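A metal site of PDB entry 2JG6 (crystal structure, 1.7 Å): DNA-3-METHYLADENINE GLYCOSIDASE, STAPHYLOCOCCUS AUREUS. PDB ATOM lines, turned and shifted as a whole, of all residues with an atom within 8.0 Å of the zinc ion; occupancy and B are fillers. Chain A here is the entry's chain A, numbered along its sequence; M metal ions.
ND1 of His 17 lies within hydrogen-bond range of OD1 of Asp 18, at 2.8 Å. A ring nitrogen (NE2) of His 175 sits at hydrogen-bond distance from the backbone carbonyl oxygen (O) of Trp 21. The backbone carbonyl oxygen (O) of His 175 sits at hydrogen-bond distance from the side-chain amino group (NZ) of Lys 182, 3.2 Å away. The backbone NH (N) of His 175 sits at hydrogen-bond distance from the side-chain carboxylate (OD1) of Asp 173, at 2.9 Å. The side-chain sulfur of Cys 179 sits close to the backbone NH of Ser 181 (3.3 Å). The side-chain sulfur (SG) of Cys 4 sits close to the backbone NH (N) of Leu 176, at 3.3 Å. O of Cys 4 sits at hydrogen-bond distance from NH2 of Arg 135 (3.0 Å).
The nearest printed residue that does not touch the zinc ion is Ser 181 (4.4 Å).
The zinc ion is bound by NE2 of His 17 (2.1 Å), ND1 of His 175 (2.1 Å), SG of Cys 179 (2.3 Å) and SG of Cys 4 (2.3 Å). The zinc ion has four donor atoms within binding distance.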
ATOM      1  N   MET A   1       5.709  -7.555 -17.715  1.00  0.00           N
ATOM      2  CA  MET A   1       6.400  -7.083 -16.477  1.00  0.00           C
ATOM      3  C   MET A   1       7.909  -7.192 -16.624  1.00  0.00           C
ATOM      4  O   MET A   1       8.455  -8.277 -16.877  1.00  0.00           O
ATOM      5  CB  MET A   1       5.899  -7.823 -15.225  1.00  0.00           C
ATOM      6  CG  MET A   1       6.848  -7.791 -14.024  1.00  0.00           C
ATOM      7  SD  MET A   1       6.060  -8.241 -12.461  1.00  0.00           S
ATOM      8  CE  MET A   1       5.171  -6.722 -12.108  1.00  0.00           C
ATOM      9  N   ASN A   2       8.557  -6.044 -16.477  1.00  0.00           N
ATOM     10  CA  ASN A   2       9.997  -5.925 -16.612  1.00  0.00           C
ATOM     11  C   ASN A   2      10.760  -6.795 -15.628  1.00  0.00           C
ATOM     12  O   ASN A   2      11.713  -7.489 -16.011  1.00  0.00           O
ATOM     13  CB  ASN A   2      10.401  -4.465 -16.422  1.00  0.00           C
ATOM     14  CG  ASN A   2      11.896  -4.271 -16.432  1.00  0.00           C
ATOM     15  OD1 ASN A   2      12.562  -4.550 -17.437  1.00  0.00           O
ATOM     16  ND2 ASN A   2      12.442  -3.812 -15.317  1.00  0.00           N
ATOM     17  N   GLU A   3      10.329  -6.769 -14.369  1.00  0.00           N
ATOM     18  CA  GLU A   3      10.967  -7.576 -13.322  1.00  0.00           C
ATOM     19  C   GLU A   3      10.933  -9.043 -13.679  1.00  0.00           C
ATOM     20  O   GLU A   3      11.943  -9.747 -13.571  1.00  0.00           O
ATOM     21  CB  GLU A   3      10.301  -7.366 -11.961  1.00  0.00           C
ATOM     22  CG  GLU A   3      11.019  -8.125 -10.853  1.00  0.00           C
ATOM     23  CD  GLU A   3      10.388  -7.987  -9.500  1.00  0.00           C
ATOM     24  OE1 GLU A   3       9.385  -7.256  -9.345  1.00  0.00           O
ATOM     25  OE2 GLU A   3      10.921  -8.626  -8.562  1.00  0.00           O
ATOM     26  N   CYS A   4       9.761  -9.499 -14.109  1.00  0.00           N
ATOM     27  CA  CYS A   4       9.579 -10.906 -14.458  1.00  0.00           C
ATOM     28  C   CYS A   4      10.465 -11.334 -15.621  1.00  0.00           C
ATOM     29  O   CYS A   4      11.036 -12.422 -15.588  1.00  0.00           O
ATOM     30  CB  CYS A   4       8.113 -11.181 -14.763  1.00  0.00           C
ATOM     31  SG  CYS A   4       7.785 -12.955 -14.971  1.00  0.00           S
ATOM     32  N   ALA A   5      10.595 -10.458 -16.617  1.00  0.00           N
ATOM     33  CA  ALA A   5      11.411 -10.752 -17.802  1.00  0.00           C
ATOM     34  C   ALA A   5      12.905 -10.446 -17.620  1.00  0.00           C
ATOM     35  O   ALA A   5      13.599 -10.029 -18.572  1.00  0.00           O
ATOM     36  CB  ALA A   5      10.845  -9.997 -18.996  1.00  0.00           C
ATOM     37  N   PHE A   6      13.395 -10.611 -16.387  1.00  0.00           N
ATOM     38  CA  PHE A   6      14.828 -10.491 -16.059  1.00  0.00           C
ATOM     39  C   PHE A   6      15.435  -9.107 -16.372  1.00  0.00           C
ATOM     40  O   PHE A   6      16.655  -8.970 -16.571  1.00  0.00           O
ATOM     41  CB  PHE A   6      15.635 -11.603 -16.750  1.00  0.00           C
ATOM     42  CG  PHE A   6      15.184 -12.994 -16.400  1.00  0.00           C
ATOM     43  CD1 PHE A   6      15.677 -13.627 -15.263  1.00  0.00           C
ATOM     44  CD2 PHE A   6      14.265 -13.668 -17.211  1.00  0.00           C
ATOM     45  CE1 PHE A   6      15.255 -14.930 -14.930  1.00  0.00           C
ATOM     46  CE2 PHE A   6      13.844 -14.961 -16.900  1.00  0.00           C
ATOM     47  CZ  PHE A   6      14.335 -15.595 -15.745  1.00  0.00           C
ATOM     48  N   HIS A  17       9.386 -13.849 -23.771  1.00  0.00           N
ATOM     49  CA  HIS A  17       8.847 -13.873 -22.424  1.00  0.00           C
ATOM     50  C   HIS A  17       7.315 -13.841 -22.428  1.00  0.00           C
ATOM     51  O   HIS A  17       6.668 -14.506 -21.608  1.00  0.00           O
ATOM     52  CB  HIS A  17       9.331 -12.688 -21.581  1.00  0.00           C
ATOM     53  CG  HIS A  17       8.505 -12.484 -20.350  1.00  0.00           C
ATOM     54  ND1 HIS A  17       7.411 -11.647 -20.331  1.00  0.00           N
ATOM     55  CD2 HIS A  17       8.547 -13.086 -19.144  1.00  0.00           C
ATOM     56  CE1 HIS A  17       6.836 -11.713 -19.135  1.00  0.00           C
ATOM     57  NE2 HIS A  17       7.512 -12.575 -18.401  1.00  0.00           N
ATOM     58  N   ASP A  18       6.765 -13.033 -23.339  1.00  0.00           N
ATOM     59  CA  ASP A  18       5.337 -12.740 -23.384  1.00  0.00           C
ATOM     60  C   ASP A  18       4.512 -13.848 -24.030  1.00  0.00           C
ATOM     61  O   ASP A  18       3.342 -14.016 -23.684  1.00  0.00           O
ATOM     62  CB  ASP A  18       5.075 -11.451 -24.175  1.00  0.00           C
ATOM     63  CG  ASP A  18       5.458 -10.175 -23.417  1.00  0.00           C
ATOM     64  OD1 ASP A  18       5.895 -10.247 -22.253  1.00  0.00           O
ATOM     65  OD2 ASP A  18       5.300  -9.092 -24.008  1.00  0.00           O
ATOM     66  N   TRP A  21       7.648 -18.310 -23.177  1.00  0.00           N
ATOM     67  CA  TRP A  21       8.208 -18.738 -21.901  1.00  0.00           C
ATOM     68  C   TRP A  21       7.107 -18.968 -20.868  1.00  0.00           C
ATOM     69  O   TRP A  21       6.304 -18.078 -20.595  1.00  0.00           O
ATOM     70  CB  TRP A  21       9.185 -17.689 -21.390  1.00  0.00           C
ATOM     71  CG  TRP A  21      10.006 -18.122 -20.203  1.00  0.00           C
ATOM     72  CD1 TRP A  21      11.108 -18.954 -20.233  1.00  0.00           C
ATOM     73  CD2 TRP A  21       9.839 -17.709 -18.853  1.00  0.00           C
ATOM     74  NE1 TRP A  21      11.611 -19.097 -18.951  1.00  0.00           N
ATOM     75  CE2 TRP A  21      10.863 -18.338 -18.095  1.00  0.00           C
ATOM     76  CE3 TRP A  21       8.924 -16.879 -18.193  1.00  0.00           C
ATOM     77  CZ2 TRP A  21      10.992 -18.157 -16.711  1.00  0.00           C
ATOM     78  CZ3 TRP A  21       9.055 -16.697 -16.826  1.00  0.00           C
ATOM     79  CH2 TRP A  21      10.082 -17.332 -16.097  1.00  0.00           C
ATOM     80  N   GLY A  22       7.065 -20.172 -20.300  1.00  0.00           N
ATOM     81  CA  GLY A  22       6.131 -20.447 -19.198  1.00  0.00           C
ATOM     82  C   GLY A  22       4.702 -20.794 -19.620  1.00  0.00           C
ATOM     83  O   GLY A  22       3.866 -21.091 -18.754  1.00  0.00           O
ATOM     84  N   GLN A  23       4.413 -20.720 -20.916  1.00  0.00           N
ATOM     85  CA  GLN A  23       3.071 -21.116 -21.409  1.00  0.00           C
ATOM     86  C   GLN A  23       3.031 -22.624 -21.624  1.00  0.00           C
ATOM     87  O   GLN A  23       3.839 -23.148 -22.387  1.00  0.00           O
ATOM     88  CB  GLN A  23       2.734 -20.411 -22.721  1.00  0.00           C
ATOM     89  CG  GLN A  23       2.883 -18.890 -22.688  1.00  0.00           C
ATOM     90  CD  GLN A  23       1.971 -18.227 -21.677  1.00  0.00           C
ATOM     91  OE1 GLN A  23       0.875 -18.738 -21.355  1.00  0.00           O
ATOM     92  NE2 GLN A  23       2.398 -17.075 -21.171  1.00  0.00           N
ATOM     93  N   ARG A 135      13.468 -16.498  -7.443  1.00  0.00           N
ATOM     94  CA  ARG A 135      13.677 -17.588  -8.403  1.00  0.00           C
ATOM     95  C   ARG A 135      14.910 -18.426  -8.115  1.00  0.00           C
ATOM     96  O   ARG A 135      15.992 -17.900  -7.856  1.00  0.00           O
ATOM     97  CB  ARG A 135      13.743 -17.037  -9.817  1.00  0.00           C
ATOM     98  CG  ARG A 135      12.448 -16.437 -10.315  1.00  0.00           C
ATOM     99  CD  ARG A 135      12.516 -16.410 -11.799  1.00  0.00           C
ATOM    100  NE  ARG A 135      11.307 -15.906 -12.423  1.00  0.00           N
ATOM    101  CZ  ARG A 135      11.225 -14.760 -13.097  1.00  0.00           C
ATOM    102  NH1 ARG A 135      12.299 -13.962 -13.247  1.00  0.00           N
ATOM    103  NH2 ARG A 135      10.071 -14.421 -13.632  1.00  0.00           N
ATOM    104  N   ASP A 173       5.703 -22.956 -13.855  1.00  0.00           N
ATOM    105  CA  ASP A 173       5.328 -21.579 -14.123  1.00  0.00           C
ATOM    106  C   ASP A 173       6.143 -20.705 -13.171  1.00  0.00           C
ATOM    107  O   ASP A 173       5.871 -20.657 -11.961  1.00  0.00           O
ATOM    108  CB  ASP A 173       3.821 -21.385 -13.918  1.00  0.00           C
ATOM    109  CG  ASP A 173       3.390 -19.923 -13.971  1.00  0.00           C
ATOM    110  OD1 ASP A 173       4.238 -19.029 -14.193  1.00  0.00           O
ATOM    111  OD2 ASP A 173       2.187 -19.651 -13.771  1.00  0.00           O
ATOM    112  N   ALA A 174       7.146 -20.035 -13.729  1.00  0.00           N
ATOM    113  CA  ALA A 174       8.000 -19.122 -12.963  1.00  0.00           C
ATOM    114  C   ALA A 174       7.689 -17.636 -13.185  1.00  0.00           C
ATOM    115  O   ALA A 174       8.468 -16.763 -12.781  1.00  0.00           O
ATOM    116  CB  ALA A 174       9.466 -19.397 -13.269  1.00  0.00           C
ATOM    117  N   HIS A 175       6.554 -17.338 -13.843  1.00  0.00           N
ATOM    118  CA  HIS A 175       6.127 -15.947 -13.969  1.00  0.00           C
ATOM    119  C   HIS A 175       5.759 -15.370 -12.610  1.00  0.00           C
ATOM    120  O   HIS A 175       5.213 -16.089 -11.761  1.00  0.00           O
ATOM    121  CB  HIS A 175       4.895 -15.825 -14.883  1.00  0.00           C
ATOM    122  CG  HIS A 175       5.197 -15.961 -16.345  1.00  0.00           C
ATOM    123  ND1 HIS A 175       5.660 -14.916 -17.119  1.00  0.00           N
ATOM    124  CD2 HIS A 175       5.072 -17.023 -17.169  1.00  0.00           C
ATOM    125  CE1 HIS A 175       5.819 -15.343 -18.359  1.00  0.00           C
ATOM    126  NE2 HIS A 175       5.458 -16.619 -18.420  1.00  0.00           N
ATOM    127  N   LEU A 176       6.043 -14.093 -12.422  1.00  0.00           N
ATOM    128  CA  LEU A 176       5.697 -13.417 -11.172  1.00  0.00           C
ATOM    129  C   LEU A 176       4.198 -13.208 -11.076  1.00  0.00           C
ATOM    130  O   LEU A 176       3.514 -13.074 -12.100  1.00  0.00           O
ATOM    131  CB  LEU A 176       6.445 -12.085 -11.036  1.00  0.00           C
ATOM    132  CG  LEU A 176       7.970 -12.144 -11.220  1.00  0.00           C
ATOM    133  CD1 LEU A 176       8.607 -10.775 -10.969  1.00  0.00           C
ATOM    134  CD2 LEU A 176       8.606 -13.204 -10.303  1.00  0.00           C
ATOM    135  N   LYS A 177       3.700 -13.155  -9.838  1.00  0.00           N
ATOM    136  CA  LYS A 177       2.267 -13.092  -9.571  1.00  0.00           C
ATOM    137  C   LYS A 177       1.589 -11.984 -10.349  1.00  0.00           C
ATOM    138  O   LYS A 177       0.481 -12.176 -10.863  1.00  0.00           O
ATOM    139  CB  LYS A 177       2.024 -12.897  -8.083  1.00  0.00           C
ATOM    140  CG  LYS A 177       0.552 -12.700  -7.713  1.00  0.00           C
ATOM    141  CD  LYS A 177       0.324 -12.685  -6.211  1.00  0.00           C
ATOM    142  CE  LYS A 177       1.064 -11.518  -5.533  1.00  0.00           C
ATOM    143  NZ  LYS A 177       0.691 -10.163  -6.092  1.00  0.00           N
ATOM    144  N   ASP A 178       2.251 -10.827 -10.450  1.00  0.00           N
ATOM    145  CA  ASP A 178       1.676  -9.668 -11.112  1.00  0.00           C
ATOM    146  C   ASP A 178       2.096  -9.486 -12.564  1.00  0.00           C
ATOM    147  O   ASP A 178       1.844  -8.435 -13.170  1.00  0.00           O
ATOM    148  CB  ASP A 178       1.985  -8.408 -10.308  1.00  0.00           C
ATOM    149  CG  ASP A 178       1.208  -8.356  -9.006  1.00  0.00           C
ATOM    150  OD1 ASP A 178       0.089  -8.935  -8.934  1.00  0.00           O
ATOM    151  OD2 ASP A 178       1.704  -7.729  -8.048  1.00  0.00           O
ATOM    152  N   CYS A 179       2.752 -10.484 -13.145  1.00  0.00           N
ATOM    153  CA  CYS A 179       3.101 -10.407 -14.562  1.00  0.00           C
ATOM    154  C   CYS A 179       1.858 -10.642 -15.416  1.00  0.00           C
ATOM    155  O   CYS A 179       1.156 -11.636 -15.187  1.00  0.00           O
ATOM    156  CB  CYS A 179       4.152 -11.441 -14.916  1.00  0.00           C
ATOM    157  SG  CYS A 179       4.623 -11.403 -16.656  1.00  0.00           S
ATOM    158  N   PRO A 180       1.620  -9.759 -16.413  1.00  0.00           N
ATOM    159  CA  PRO A 180       0.512  -9.883 -17.359  1.00  0.00           C
ATOM    160  C   PRO A 180       0.540 -11.185 -18.155  1.00  0.00           C
ATOM    161  O   PRO A 180      -0.487 -11.586 -18.692  1.00  0.00           O
ATOM    162  CB  PRO A 180       0.724  -8.700 -18.320  1.00  0.00           C
ATOM    163  CG  PRO A 180       1.538  -7.727 -17.549  1.00  0.00           C
ATOM    164  CD  PRO A 180       2.436  -8.560 -16.696  1.00  0.00           C
ATOM    165  N   SER A 181       1.714 -11.811 -18.249  1.00  0.00           N
ATOM    166  CA  SER A 181       1.851 -13.041 -19.025  1.00  0.00           C
ATOM    167  C   SER A 181       1.730 -14.307 -18.189  1.00  0.00           C
ATOM    168  O   SER A 181       1.908 -15.399 -18.722  1.00  0.00           O
ATOM    169  CB  SER A 181       3.171 -13.057 -19.793  1.00  0.00           C
ATOM    170  OG  SER A 181       3.154 -12.037 -20.782  1.00  0.00           O
ATOM    171  N   LYS A 182       1.443 -14.170 -16.894  1.00  0.00           N
ATOM    172  CA  LYS A 182       1.316 -15.367 -16.043  1.00  0.00           C
ATOM    173  C   LYS A 182       0.088 -16.173 -16.468  1.00  0.00           C
ATOM    174  O   LYS A 182      -1.024 -15.635 -16.501  1.00  0.00           O
ATOM    175  CB  LYS A 182       1.239 -15.007 -14.549  1.00  0.00           C
ATOM    176  CG  LYS A 182       1.279 -16.268 -13.676  1.00  0.00           C
ATOM    177  CD  LYS A 182       1.210 -16.001 -12.182  1.00  0.00           C
ATOM    178  CE  LYS A 182       1.244 -17.324 -11.440  1.00  0.00           C
ATOM    179  NZ  LYS A 182       2.602 -17.933 -11.448  1.00  0.00           N
ATOM    180  N   PRO A 183       0.281 -17.452 -16.830  1.00  0.00           N
ATOM    181  CA  PRO A 183      -0.881 -18.231 -17.319  1.00  0.00           C
ATOM    182  C   PRO A 183      -1.868 -18.577 -16.207  1.00  0.00           C
ATOM    183  O   PRO A 183      -1.485 -18.674 -15.038  1.00  0.00           O
ATOM    184  CB  PRO A 183      -0.237 -19.496 -17.904  1.00  0.00           C
ATOM    185  CG  PRO A 183       1.106 -19.595 -17.287  1.00  0.00           C
ATOM    186  CD  PRO A 183       1.539 -18.209 -16.884  1.00  0.00           C
HETATM  187 ZN    ZN M   1       6.319 -12.966 -16.770  1.00  0.00          ZN
